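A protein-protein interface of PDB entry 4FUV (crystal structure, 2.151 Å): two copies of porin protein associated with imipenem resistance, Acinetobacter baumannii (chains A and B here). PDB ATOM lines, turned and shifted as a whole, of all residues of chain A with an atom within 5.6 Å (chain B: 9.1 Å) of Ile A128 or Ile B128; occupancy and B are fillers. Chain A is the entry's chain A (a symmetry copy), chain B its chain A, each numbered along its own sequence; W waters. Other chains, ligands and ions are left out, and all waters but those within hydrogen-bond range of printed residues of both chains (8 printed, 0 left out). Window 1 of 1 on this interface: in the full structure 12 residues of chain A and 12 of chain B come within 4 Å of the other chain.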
ATOM      1  N   THR A 117       5.293  21.158  13.698  1.00  0.00           N
ATOM      2  CA  THR A 117       4.318  20.134  13.281  1.00  0.00           C
ATOM      3  C   THR A 117       4.104  18.984  14.258  1.00  0.00           C
ATOM      4  O   THR A 117       3.321  18.083  13.961  1.00  0.00           O
ATOM      5  CB  THR A 117       4.624  19.492  11.909  1.00  0.00           C
ATOM      6  OG1 THR A 117       5.699  18.563  12.066  1.00  0.00           O
ATOM      7  CG2 THR A 117       4.992  20.545  10.868  1.00  0.00           C
ATOM      8  N   ARG A 118       4.795  18.988  15.399  1.00  0.00           N
ATOM      9  CA  ARG A 118       4.670  17.869  16.330  1.00  0.00           C
ATOM     10  C   ARG A 118       3.621  18.123  17.406  1.00  0.00           C
ATOM     11  O   ARG A 118       3.421  19.260  17.858  1.00  0.00           O
ATOM     12  CB  ARG A 118       6.018  17.506  16.985  1.00  0.00           C
ATOM     13  CG  ARG A 118       7.124  17.119  16.001  1.00  0.00           C
ATOM     14  CD  ARG A 118       6.687  16.031  15.020  1.00  0.00           C
ATOM     15  NE  ARG A 118       6.329  14.786  15.699  1.00  0.00           N
ATOM     16  CZ  ARG A 118       7.192  13.805  15.956  1.00  0.00           C
ATOM     17  NH1 ARG A 118       8.467  13.934  15.603  1.00  0.00           N
ATOM     18  NH2 ARG A 118       6.787  12.698  16.573  1.00  0.00           N
ATOM     19  N   SER A 119       2.957  17.052  17.820  1.00  0.00           N
ATOM     20  CA  SER A 119       1.985  17.147  18.897  1.00  0.00           C
ATOM     21  C   SER A 119       2.656  17.152  20.271  1.00  0.00           C
ATOM     22  O   SER A 119       3.752  16.626  20.454  1.00  0.00           O
ATOM     23  CB  SER A 119       0.975  16.001  18.820  1.00  0.00           C
ATOM     24  OG  SER A 119       1.628  14.761  18.958  1.00  0.00           O
ATOM     25  N   PHE A 120       1.976  17.772  21.221  1.00  0.00           N
ATOM     26  CA  PHE A 120       2.414  17.849  22.598  1.00  0.00           C
ATOM     27  C   PHE A 120       1.155  18.123  23.404  1.00  0.00           C
ATOM     28  O   PHE A 120       0.139  18.558  22.849  1.00  0.00           O
ATOM     29  CB  PHE A 120       3.453  18.962  22.783  1.00  0.00           C
ATOM     30  CG  PHE A 120       2.930  20.359  22.490  1.00  0.00           C
ATOM     31  CD1 PHE A 120       2.770  20.797  21.183  1.00  0.00           C
ATOM     32  CD2 PHE A 120       2.619  21.232  23.526  1.00  0.00           C
ATOM     33  CE1 PHE A 120       2.292  22.070  20.916  1.00  0.00           C
ATOM     34  CE2 PHE A 120       2.144  22.520  23.259  1.00  0.00           C
ATOM     35  CZ  PHE A 120       1.984  22.934  21.965  1.00  0.00           C
ATOM     36  N   ASP A 126      -4.443  18.144  23.875  1.00  0.00           N
ATOM     37  CA  ASP A 126      -3.455  17.970  22.819  1.00  0.00           C
ATOM     38  C   ASP A 126      -3.354  19.227  21.960  1.00  0.00           C
ATOM     39  O   ASP A 126      -4.371  19.852  21.646  1.00  0.00           O
ATOM     40  CB  ASP A 126      -3.818  16.775  21.944  1.00  0.00           C
ATOM     41  CG  ASP A 126      -3.747  15.453  22.703  1.00  0.00           C
ATOM     42  OD1 ASP A 126      -2.896  15.318  23.605  1.00  0.00           O
ATOM     43  OD2 ASP A 126      -4.541  14.550  22.392  1.00  0.00           O
ATOM     44  N   PHE A 127      -2.118  19.572  21.597  1.00  0.00           N
ATOM     45  CA  PHE A 127      -1.813  20.689  20.721  1.00  0.00           C
ATOM     46  C   PHE A 127      -0.803  20.226  19.679  1.00  0.00           C
ATOM     47  O   PHE A 127      -0.079  19.265  19.900  1.00  0.00           O
ATOM     48  CB  PHE A 127      -1.201  21.852  21.503  1.00  0.00           C
ATOM     49  CG  PHE A 127      -2.156  22.535  22.439  1.00  0.00           C
ATOM     50  CD1 PHE A 127      -2.365  22.039  23.715  1.00  0.00           C
ATOM     51  CD2 PHE A 127      -2.820  23.696  22.052  1.00  0.00           C
ATOM     52  CE1 PHE A 127      -3.236  22.673  24.590  1.00  0.00           C
ATOM     53  CE2 PHE A 127      -3.691  24.337  22.913  1.00  0.00           C
ATOM     54  CZ  PHE A 127      -3.897  23.821  24.197  1.00  0.00           C
ATOM     55  N   ILE A 128      -0.760  20.917  18.544  1.00  0.00           N
ATOM     56  CA  ILE A 128       0.255  20.650  17.533  1.00  0.00           C
ATOM     57  C   ILE A 128       0.970  21.949  17.190  1.00  0.00           C
ATOM     58  O   ILE A 128       0.334  22.918  16.776  1.00  0.00           O
ATOM     59  CB  ILE A 128      -0.351  20.049  16.243  1.00  0.00           C
ATOM     60  CG1 ILE A 128      -0.663  18.558  16.444  1.00  0.00           C
ATOM     61  CG2 ILE A 128       0.618  20.216  15.071  1.00  0.00           C
ATOM     62  CD1 ILE A 128      -1.457  17.931  15.283  1.00  0.00           C
ATOM     63  N   ALA A 129       2.292  21.953  17.353  1.00  0.00           N
ATOM     64  CA  ALA A 129       3.100  23.147  17.138  1.00  0.00           C
ATOM     65  C   ALA A 129       3.066  23.610  15.680  1.00  0.00           C
ATOM     66  O   ALA A 129       3.156  22.796  14.757  1.00  0.00           O
ATOM     67  CB  ALA A 129       4.534  22.893  17.573  1.00  0.00           C
ATOM     68  N   GLY A 130       2.960  24.920  15.486  1.00  0.00           N
ATOM     69  CA  GLY A 130       2.990  25.503  14.155  1.00  0.00           C
ATOM     70  C   GLY A 130       4.360  25.447  13.506  1.00  0.00           C
ATOM     71  O   GLY A 130       5.309  24.896  14.068  1.00  0.00           O
ATOM     72  N   SER A 185       3.048  29.365  18.220  1.00  0.00           N
ATOM     73  CA  SER A 185       1.640  29.130  17.962  1.00  0.00           C
ATOM     74  C   SER A 185       1.382  27.646  17.794  1.00  0.00           C
ATOM     75  O   SER A 185       2.268  26.905  17.371  1.00  0.00           O
ATOM     76  CB  SER A 185       1.188  29.871  16.694  1.00  0.00           C
ATOM     77  OG  SER A 185       1.107  31.270  16.902  1.00  0.00           O
ATOM     78  N   ALA A 186       0.156  27.233  18.089  1.00  0.00           N
ATOM     79  CA  ALA A 186      -0.236  25.841  17.981  1.00  0.00           C
ATOM     80  C   ALA A 186      -1.694  25.727  17.568  1.00  0.00           C
ATOM     81  O   ALA A 186      -2.495  26.614  17.842  1.00  0.00           O
ATOM     82  CB  ALA A 186      -0.004  25.137  19.303  1.00  0.00           C
ATOM     83  N   VAL A 187      -2.030  24.642  16.884  1.00  0.00           N
ATOM     84  CA  VAL A 187      -3.426  24.360  16.565  1.00  0.00           C
ATOM     85  C   VAL A 187      -3.963  23.341  17.551  1.00  0.00           C
ATOM     86  O   VAL A 187      -3.192  22.597  18.171  1.00  0.00           O
ATOM     87  CB  VAL A 187      -3.583  23.815  15.144  1.00  0.00           C
ATOM     88  CG1 VAL A 187      -3.024  24.817  14.137  1.00  0.00           C
ATOM     89  CG2 VAL A 187      -2.868  22.469  15.015  1.00  0.00           C
ATOM     90  N   THR A 188      -5.286  23.287  17.685  1.00  0.00           N
ATOM     91  CA  THR A 188      -5.910  22.410  18.670  1.00  0.00           C
ATOM     92  C   THR A 188      -7.405  22.298  18.373  1.00  0.00           C
ATOM     93  O   THR A 188      -7.920  23.072  17.588  1.00  0.00           O
ATOM     94  CB  THR A 188      -5.716  22.988  20.082  1.00  0.00           C
ATOM     95  OG1 THR A 188      -5.929  21.968  21.061  1.00  0.00           O
ATOM     96  CG2 THR A 188      -6.676  24.178  20.334  1.00  0.00           C
ATOM     97  N   THR A 189      -8.097  21.334  18.976  1.00  0.00           N
ATOM     98  CA  THR A 189      -9.548  21.300  18.852  1.00  0.00           C
ATOM     99  C   THR A 189     -10.182  21.245  20.219  1.00  0.00           C
ATOM    100  O   THR A 189     -11.391  21.141  20.337  1.00  0.00           O
ATOM    101  CB  THR A 189     -10.078  20.133  17.995  1.00  0.00           C
ATOM    102  OG1 THR A 189      -9.567  18.899  18.515  1.00  0.00           O
ATOM    103  CG2 THR A 189      -9.664  20.299  16.525  1.00  0.00           C
ATOM    104  N   VAL B 114     -10.449   7.439  16.872  1.00  0.00           N
ATOM    105  CA  VAL B 114      -9.756   8.481  17.620  1.00  0.00           C
ATOM    106  C   VAL B 114     -10.760   9.391  18.325  1.00  0.00           C
ATOM    107  O   VAL B 114     -11.619   9.978  17.673  1.00  0.00           O
ATOM    108  CB  VAL B 114      -8.838   9.299  16.681  1.00  0.00           C
ATOM    109  CG1 VAL B 114      -8.076  10.378  17.449  1.00  0.00           C
ATOM    110  CG2 VAL B 114      -7.874   8.368  15.954  1.00  0.00           C
ATOM    111  N   ASP B 115     -10.668   9.485  19.653  1.00  0.00           N
ATOM    112  CA  ASP B 115     -11.538  10.379  20.418  1.00  0.00           C
ATOM    113  C   ASP B 115     -11.384  11.811  19.948  1.00  0.00           C
ATOM    114  O   ASP B 115     -10.308  12.222  19.506  1.00  0.00           O
ATOM    115  CB  ASP B 115     -11.204  10.366  21.910  1.00  0.00           C
ATOM    116  CG  ASP B 115     -11.618   9.091  22.601  1.00  0.00           C
ATOM    117  OD1 ASP B 115     -12.486   8.366  22.066  1.00  0.00           O
ATOM    118  OD2 ASP B 115     -11.075   8.834  23.698  1.00  0.00           O
ATOM    119  N   ALA B 116     -12.478  12.560  20.056  1.00  0.00           N
ATOM    120  CA  ALA B 116     -12.485  13.993  19.829  1.00  0.00           C
ATOM    121  C   ALA B 116     -11.360  14.682  20.610  1.00  0.00           C
ATOM    122  O   ALA B 116     -11.153  14.383  21.784  1.00  0.00           O
ATOM    123  CB  ALA B 116     -13.831  14.565  20.243  1.00  0.00           C
ATOM    124  N   THR B 117     -10.667  15.607  19.936  1.00  0.00           N
ATOM    125  CA  THR B 117      -9.575  16.435  20.478  1.00  0.00           C
ATOM    126  C   THR B 117      -8.247  15.722  20.695  1.00  0.00           C
ATOM    127  O   THR B 117      -7.300  16.349  21.168  1.00  0.00           O
ATOM    128  CB  THR B 117      -9.919  17.139  21.811  1.00  0.00           C
ATOM    129  OG1 THR B 117      -9.862  16.177  22.866  1.00  0.00           O
ATOM    130  CG2 THR B 117     -11.301  17.782  21.764  1.00  0.00           C
ATOM    131  N   ARG B 118      -8.165  14.428  20.382  1.00  0.00           N
ATOM    132  CA  ARG B 118      -6.930  13.692  20.641  1.00  0.00           C
ATOM    133  C   ARG B 118      -6.012  13.654  19.426  1.00  0.00           C
ATOM    134  O   ARG B 118      -6.465  13.611  18.273  1.00  0.00           O
ATOM    135  CB  ARG B 118      -7.204  12.257  21.138  1.00  0.00           C
ATOM    136  CG  ARG B 118      -8.027  12.172  22.424  1.00  0.00           C
ATOM    137  CD  ARG B 118      -7.457  13.036  23.549  1.00  0.00           C
ATOM    138  NE  ARG B 118      -6.106  12.625  23.933  1.00  0.00           N
ATOM    139  CZ  ARG B 118      -5.846  11.725  24.880  1.00  0.00           C
ATOM    140  NH1 ARG B 118      -6.844  11.137  25.529  1.00  0.00           N
ATOM    141  NH2 ARG B 118      -4.588  11.409  25.177  1.00  0.00           N
ATOM    142  N   SER B 119      -4.712  13.663  19.692  1.00  0.00           N
ATOM    143  CA  SER B 119      -3.730  13.553  18.625  1.00  0.00           C
ATOM    144  C   SER B 119      -3.538  12.103  18.177  1.00  0.00           C
ATOM    145  O   SER B 119      -3.754  11.161  18.937  1.00  0.00           O
ATOM    146  CB  SER B 119      -2.388  14.143  19.059  1.00  0.00           C
ATOM    147  OG  SER B 119      -1.878  13.439  20.167  1.00  0.00           O
ATOM    148  N   PHE B 120      -3.140  11.955  16.925  1.00  0.00           N
ATOM    149  CA  PHE B 120      -2.856  10.672  16.322  1.00  0.00           C
ATOM    150  C   PHE B 120      -1.942  10.974  15.146  1.00  0.00           C
ATOM    151  O   PHE B 120      -1.872  12.121  14.686  1.00  0.00           O
ATOM    152  CB  PHE B 120      -4.147   9.980  15.867  1.00  0.00           C
ATOM    153  CG  PHE B 120      -4.907  10.728  14.784  1.00  0.00           C
ATOM    154  CD1 PHE B 120      -5.676  11.841  15.096  1.00  0.00           C
ATOM    155  CD2 PHE B 120      -4.864  10.301  13.462  1.00  0.00           C
ATOM    156  CE1 PHE B 120      -6.367  12.524  14.110  1.00  0.00           C
ATOM    157  CE2 PHE B 120      -5.568  10.985  12.465  1.00  0.00           C
ATOM    158  CZ  PHE B 120      -6.314  12.085  12.788  1.00  0.00           C
ATOM    159  N   ARG B 121      -1.251   9.956  14.654  1.00  0.00           N
ATOM    160  CA  ARG B 121      -0.192  10.156  13.660  1.00  0.00           C
ATOM    161  C   ARG B 121      -0.479   9.323  12.418  1.00  0.00           C
ATOM    162  O   ARG B 121      -0.809   8.142  12.528  1.00  0.00           O
ATOM    163  CB  ARG B 121       1.158   9.741  14.258  1.00  0.00           C
ATOM    164  CG  ARG B 121       2.396  10.122  13.456  1.00  0.00           C
ATOM    165  CD  ARG B 121       3.637   9.974  14.363  1.00  0.00           C
ATOM    166  NE  ARG B 121       4.906  10.240  13.684  1.00  0.00           N
ATOM    167  CZ  ARG B 121       5.367  11.451  13.382  1.00  0.00           C
ATOM    168  NH1 ARG B 121       4.655  12.535  13.673  1.00  0.00           N
ATOM    169  NH2 ARG B 121       6.543  11.581  12.774  1.00  0.00           N
ATOM    170  N   VAL B 122      -0.376   9.939  11.242  1.00  0.00           N
ATOM    171  CA  VAL B 122      -0.603   9.224   9.987  1.00  0.00           C
ATOM    172  C   VAL B 122       0.508   9.575   9.004  1.00  0.00           C
ATOM    173  O   VAL B 122       0.762  10.756   8.738  1.00  0.00           O
ATOM    174  CB  VAL B 122      -1.988   9.551   9.366  1.00  0.00           C
ATOM    175  CG1 VAL B 122      -2.198   8.762   8.076  1.00  0.00           C
ATOM    176  CG2 VAL B 122      -3.111   9.243  10.354  1.00  0.00           C
ATOM    177  N   GLN B 125       3.035  12.149  10.203  1.00  0.00           N
ATOM    178  CA  GLN B 125       2.529  13.494  10.434  1.00  0.00           C
ATOM    179  C   GLN B 125       1.501  13.448  11.555  1.00  0.00           C
ATOM    180  O   GLN B 125       0.677  12.526  11.625  1.00  0.00           O
ATOM    181  CB  GLN B 125       1.919  14.087   9.164  1.00  0.00           C
ATOM    182  CG  GLN B 125       1.408  15.507   9.352  1.00  0.00           C
ATOM    183  CD  GLN B 125       0.896  16.143   8.070  1.00  0.00           C
ATOM    184  OE1 GLN B 125       1.466  15.952   6.994  1.00  0.00           O
ATOM    185  NE2 GLN B 125      -0.175  16.926   8.186  1.00  0.00           N
ATOM    186  N   ASP B 126       1.580  14.423  12.451  1.00  0.00           N
ATOM    187  CA  ASP B 126       0.652  14.497  13.570  1.00  0.00           C
ATOM    188  C   ASP B 126      -0.631  15.216  13.163  1.00  0.00           C
ATOM    189  O   ASP B 126      -0.585  16.213  12.436  1.00  0.00           O
ATOM    190  CB  ASP B 126       1.296  15.221  14.747  1.00  0.00           C
ATOM    191  CG  ASP B 126       2.478  14.451  15.330  1.00  0.00           C
ATOM    192  OD1 ASP B 126       2.454  13.203  15.314  1.00  0.00           O
ATOM    193  OD2 ASP B 126       3.427  15.095  15.806  1.00  0.00           O
ATOM    194  N   PHE B 127      -1.757  14.687  13.642  1.00  0.00           N
ATOM    195  CA  PHE B 127      -3.075  15.262  13.434  1.00  0.00           C
ATOM    196  C   PHE B 127      -3.815  15.273  14.766  1.00  0.00           C
ATOM    197  O   PHE B 127      -3.500  14.498  15.658  1.00  0.00           O
ATOM    198  CB  PHE B 127      -3.886  14.433  12.439  1.00  0.00           C
ATOM    199  CG  PHE B 127      -3.374  14.489  11.028  1.00  0.00           C
ATOM    200  CD1 PHE B 127      -2.361  13.641  10.613  1.00  0.00           C
ATOM    201  CD2 PHE B 127      -3.932  15.370  10.105  1.00  0.00           C
ATOM    202  CE1 PHE B 127      -1.892  13.679   9.308  1.00  0.00           C
ATOM    203  CE2 PHE B 127      -3.474  15.420   8.803  1.00  0.00           C
ATOM    204  CZ  PHE B 127      -2.445  14.560   8.400  1.00  0.00           C
ATOM    205  N   ILE B 128      -4.801  16.157  14.892  1.00  0.00           N
ATOM    206  CA  ILE B 128      -5.662  16.169  16.066  1.00  0.00           C
ATOM    207  C   ILE B 128      -7.115  16.103  15.618  1.00  0.00           C
ATOM    208  O   ILE B 128      -7.573  16.960  14.861  1.00  0.00           O
ATOM    209  CB  ILE B 128      -5.454  17.435  16.929  1.00  0.00           C
ATOM    210  CG1 ILE B 128      -4.173  17.306  17.768  1.00  0.00           C
ATOM    211  CG2 ILE B 128      -6.652  17.651  17.856  1.00  0.00           C
ATOM    212  CD1 ILE B 128      -3.780  18.603  18.498  1.00  0.00           C
ATOM    213  N   ALA B 129      -7.834  15.092  16.101  1.00  0.00           N
ATOM    214  CA  ALA B 129      -9.216  14.856  15.701  1.00  0.00           C
ATOM    215  C   ALA B 129     -10.141  15.997  16.131  1.00  0.00           C
ATOM    216  O   ALA B 129     -10.045  16.499  17.254  1.00  0.00           O
ATOM    217  CB  ALA B 129      -9.709  13.538  16.275  1.00  0.00           C
ATOM    218  N   GLY B 130     -11.048  16.380  15.240  1.00  0.00           N
ATOM    219  CA  GLY B 130     -12.038  17.401  15.542  1.00  0.00           C
ATOM    220  C   GLY B 130     -13.098  16.936  16.524  1.00  0.00           C
ATOM    221  O   GLY B 130     -13.046  15.815  17.035  1.00  0.00           O
ATOM    222  N   ALA B 131     -14.068  17.811  16.776  1.00  0.00           N
ATOM    223  CA  ALA B 131     -15.113  17.588  17.768  1.00  0.00           C
ATOM    224  C   ALA B 131     -15.903  16.295  17.577  1.00  0.00           C
ATOM    225  O   ALA B 131     -16.446  15.751  18.535  1.00  0.00           O
ATOM    226  CB  ALA B 131     -16.071  18.796  17.801  1.00  0.00           C
ATOM    227  N   ASP B 132     -15.976  15.805  16.346  1.00  0.00           N
ATOM    228  CA  ASP B 132     -16.766  14.612  16.067  1.00  0.00           C
ATOM    229  C   ASP B 132     -15.921  13.355  15.984  1.00  0.00           C
ATOM    230  O   ASP B 132     -16.427  12.288  15.651  1.00  0.00           O
ATOM    231  CB  ASP B 132     -17.555  14.782  14.779  1.00  0.00           C
ATOM    232  CG  ASP B 132     -18.619  15.852  14.893  1.00  0.00           C
ATOM    233  OD1 ASP B 132     -19.141  16.045  16.014  1.00  0.00           O
ATOM    234  OD2 ASP B 132     -18.918  16.505  13.868  1.00  0.00           O
ATOM    235  N   GLY B 133     -14.633  13.480  16.284  1.00  0.00           N
ATOM    236  CA  GLY B 133     -13.740  12.333  16.265  1.00  0.00           C
ATOM    237  C   GLY B 133     -13.282  11.937  14.876  1.00  0.00           C
ATOM    238  O   GLY B 133     -13.695  12.513  13.874  1.00  0.00           O
ATOM    239  N   VAL B 134     -12.401  10.949  14.817  1.00  0.00           N
ATOM    240  CA  VAL B 134     -11.895  10.464  13.544  1.00  0.00           C
ATOM    241  C   VAL B 134     -11.834   8.942  13.563  1.00  0.00           C
ATOM    242  O   VAL B 134     -11.462   8.340  14.560  1.00  0.00           O
ATOM    243  CB  VAL B 134     -10.509  11.054  13.228  1.00  0.00           C
ATOM    244  CG1 VAL B 134      -9.879  10.349  12.039  1.00  0.00           C
ATOM    245  CG2 VAL B 134     -10.621  12.582  12.962  1.00  0.00           C
ATOM    246  N   GLY B 184     -14.140  11.779   9.186  1.00  0.00           N
ATOM    247  CA  GLY B 184     -13.995  12.794  10.211  1.00  0.00           C
ATOM    248  C   GLY B 184     -12.988  13.854   9.815  1.00  0.00           C
ATOM    249  O   GLY B 184     -12.267  13.720   8.829  1.00  0.00           O
ATOM    250  N   SER B 185     -12.922  14.919  10.593  1.00  0.00           N
ATOM    251  CA  SER B 185     -12.036  16.028  10.290  1.00  0.00           C
ATOM    252  C   SER B 185     -10.952  16.130  11.344  1.00  0.00           C
ATOM    253  O   SER B 185     -11.161  15.740  12.492  1.00  0.00           O
ATOM    254  CB  SER B 185     -12.818  17.349  10.236  1.00  0.00           C
ATOM    255  OG  SER B 185     -13.627  17.435   9.075  1.00  0.00           O
ATOM    256  N   ALA B 186      -9.815  16.692  10.954  1.00  0.00           N
ATOM    257  CA  ALA B 186      -8.686  16.853  11.851  1.00  0.00           C
ATOM    258  C   ALA B 186      -7.922  18.123  11.522  1.00  0.00           C
ATOM    259  O   ALA B 186      -7.925  18.583  10.385  1.00  0.00           O
ATOM    260  CB  ALA B 186      -7.776  15.646  11.754  1.00  0.00           C
ATOM    261  N   VAL B 187      -7.284  18.706  12.529  1.00  0.00           N
ATOM    262  CA  VAL B 187      -6.401  19.844  12.298  1.00  0.00           C
ATOM    263  C   VAL B 187      -4.964  19.360  12.276  1.00  0.00           C
ATOM    264  O   VAL B 187      -4.651  18.292  12.818  1.00  0.00           O
ATOM    265  CB  VAL B 187      -6.556  20.909  13.386  1.00  0.00           C
ATOM    266  CG1 VAL B 187      -8.002  21.392  13.441  1.00  0.00           C
ATOM    267  CG2 VAL B 187      -6.126  20.344  14.741  1.00  0.00           C
ATOM    268  N   THR B 188      -4.082  20.151  11.670  1.00  0.00           N
ATOM    269  CA  THR B 188      -2.689  19.744  11.508  1.00  0.00           C
ATOM    270  C   THR B 188      -1.853  20.956  11.099  1.00  0.00           C
ATOM    271  O   THR B 188      -2.410  21.975  10.735  1.00  0.00           O
ATOM    272  CB  THR B 188      -2.583  18.665  10.417  1.00  0.00           C
ATOM    273  OG1 THR B 188      -1.342  17.967  10.540  1.00  0.00           O
ATOM    274  CG2 THR B 188      -2.708  19.287   9.003  1.00  0.00           C
ATOM    275  N   THR B 189      -0.527  20.862  11.175  1.00  0.00           N
ATOM    276  CA  THR B 189       0.305  21.929  10.637  1.00  0.00           C
ATOM    277  C   THR B 189       1.313  21.360   9.670  1.00  0.00           C
ATOM    278  O   THR B 189       2.154  22.078   9.158  1.00  0.00           O
ATOM    279  CB  THR B 189       1.038  22.755  11.711  1.00  0.00           C
ATOM    280  OG1 THR B 189       1.794  21.872  12.549  1.00  0.00           O
ATOM    281  CG2 THR B 189       0.043  23.563  12.558  1.00  0.00           C
ATOM    282  N   GLY B 190       1.214  20.063   9.412  1.00  0.00           N
ATOM    283  CA  GLY B 190       2.129  19.416   8.500  1.00  0.00           C
ATOM    284  C   GLY B 190       1.759  19.649   7.052  1.00  0.00           C
ATOM    285  O   GLY B 190       0.770  20.317   6.743  1.00  0.00           O
ATOM    286  N   LEU B 194      -5.208  15.187   5.965  1.00  0.00           N
ATOM    287  CA  LEU B 194      -5.513  13.852   6.482  1.00  0.00           C
ATOM    288  C   LEU B 194      -5.723  12.840   5.354  1.00  0.00           C
ATOM    289  O   LEU B 194      -5.188  11.733   5.412  1.00  0.00           O
ATOM    290  CB  LEU B 194      -6.759  13.902   7.377  1.00  0.00           C
ATOM    291  CG  LEU B 194      -7.190  12.566   7.994  1.00  0.00           C
ATOM    292  CD1 LEU B 194      -5.992  11.881   8.640  1.00  0.00           C
ATOM    293  CD2 LEU B 194      -8.282  12.796   9.025  1.00  0.00           C
HETATM  294  O   HOH W   1       0.402  12.846  17.233  1.00  0.00           O
HETATM  295  O   HOH W   2      -6.912  16.698  23.960  1.00  0.00           O
HETATM  296  O   HOH W   3       4.065  15.843  12.382  1.00  0.00           O
HETATM  297  O   HOH W   4      -2.388  12.743  23.620  1.00  0.00           O
HETATM  298  O   HOH W   5      -7.159  19.114  20.709  1.00  0.00           O
HETATM  299  O   HOH W   6       3.900  12.513  17.394  1.00  0.00           O
HETATM  300  O   HOH W   7      -0.600  15.269  21.947  1.00  0.00           O
HETATM  301  O   HOH W   8       1.168  18.682  12.263  1.00  0.00           O
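N of Ser B119 is in hydrogen-bond range of OD2 of Asp A126 (2.8 Å). The side-chain hydroxyl of Thr A189 is in hydrogen-bond range of the backbone carbonyl oxygen of Ala B129 (2.8 Å). The guanidinium group (NE) of Arg A118 is in salt-bridge range of the side-chain carboxylate (OD2) of Asp B126 (2.9 Å). NE of Arg B118 lies within salt-bridge range of OD2 of Asp A126 (2.9 Å). The side-chain carboxylate (OD2) of Asp B126 sits at hydrogen-bond distance from the backbone NH (N) of Ser A119 (2.8 Å). NE of Arg A118 sits close to NH1 of Arg B121 (3.5 Å). O of Ala A129 is in hydrogen-bond range of OG1 of Thr B189, 2.8 Å away.
The backbone NH (N) of Phe A127 sits at hydrogen-bond distance from the backbone carbonyl oxygen (O) of Phe A120. OG1 of Thr B188 sits at hydrogen-bond distance from N of Gly B190, 3.5 Å away. The backbone NH of Ala B129 lies within hydrogen-bond range of the backbone carbonyl oxygen of Arg B118 (3.0 Å). The guanidinium group of Arg B121 is in salt-bridge range of the side-chain carboxylate of Asp B126.
Water W8 lies within hydrogen-bond range of the backbone carbonyl oxygen of Thr A117 (2.8 Å), the backbone NH of Thr B189 (3.0 Å), the backbone carbonyl oxygen of Asp B126 (3.0 Å), the side-chain hydroxyl of Thr B188 (3.1 Å) and the backbone NH of Gly B190 (3.2 Å). Water W1 lies within hydrogen-bond range of OD1 of Asp B126 (2.8 Å), OG of Ser A119 (2.9 Å) and O of Phe B120 (3.5 Å).
Ile A128 touches its own counterpart, Ile B128. Ile A128 touches Thr B189, and with the chains exchanged Thr A189 touches Ile B128. Ala A129 touches Thr B189, and with the chains exchanged Thr A189 touches Ala B129. Val B187 touches its own counterpart, Val A187.
Ile A128 touches four residues of chain B. Ala A129 touches one residue of chain B. No residue of chain B comes within 4 Å of Ala A186. Of the printed residues of chain B, Val A187 touches Val B187 and Thr B189. Of the printed residues of chain A, Thr B117 touches Asp A126 (3.5 Å) and Thr A189 (3.2 Å). Phe B120 touches none of the printed residues of chain A. Of the printed residues of chain A, Phe B127 touches Ile A128. Ile B128 touches four residues of chain A. Leu B194 touches none of the printed residues of chain A. The nearest residue of chain A that does not touch Ile B128 is Val A187 (4.1 Å). The nearest printed residue of chain B that does not touch Ser A119 is Ile B128 (5.4 Å).
Of the 27 printed residues of chain B, 12 touch a printed residue of chain A. Hydrophobic or aromatic side chains of chain B within 4 Å of the printed part of chain A: Ile B128 and Val B187. Printed residues of chain A that touch a printed residue of chain B: Thr A117, Arg A118, Ser A119, Asp A126, Phe A127, Ile A128, Ala A129, Gly A130, Val A187 and Thr A189. Hydrophobic or aromatic side chains of chain A within 4 Å of the printed part of chain B: Ile A128 and Val A187. Among the printed residues, 25 pairs touch across the chains.
Among the printed residues, merely in contact across the chains: Thr A117 with Asp B126 (3.5 Å), Thr A117 with Thr B189 (3.2 Å), Thr A117 with Gly B190 (3.9 Å), Ser A119 with Ser B119 (3.8 Å), Asp A126 with Thr B117 (3.5 Å), Asp A126 with Ile B128 (3.4 Å), Phe A127 with Ile B128 (3.6 Å), Ile A128 with Asp B126 (3.4 Å), Ile A128 with Phe B127 (3.6 Å), Ile A128 with Ile B128 (3.7 Å), Ile A128 with Thr B189 (3.2 Å), Gly A130 with Thr B189 (3.9 Å), Val A187 with Val B187 (3.9 Å), Val A187 with Thr B189 (3.7 Å), Thr A189 with Thr B117 (3.2 Å), Thr A189 with Ile B128 (3.2 Å), Thr A189 with Gly B130 (3.9 Å) and Thr A189 with Val B187 (3.7 Å).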
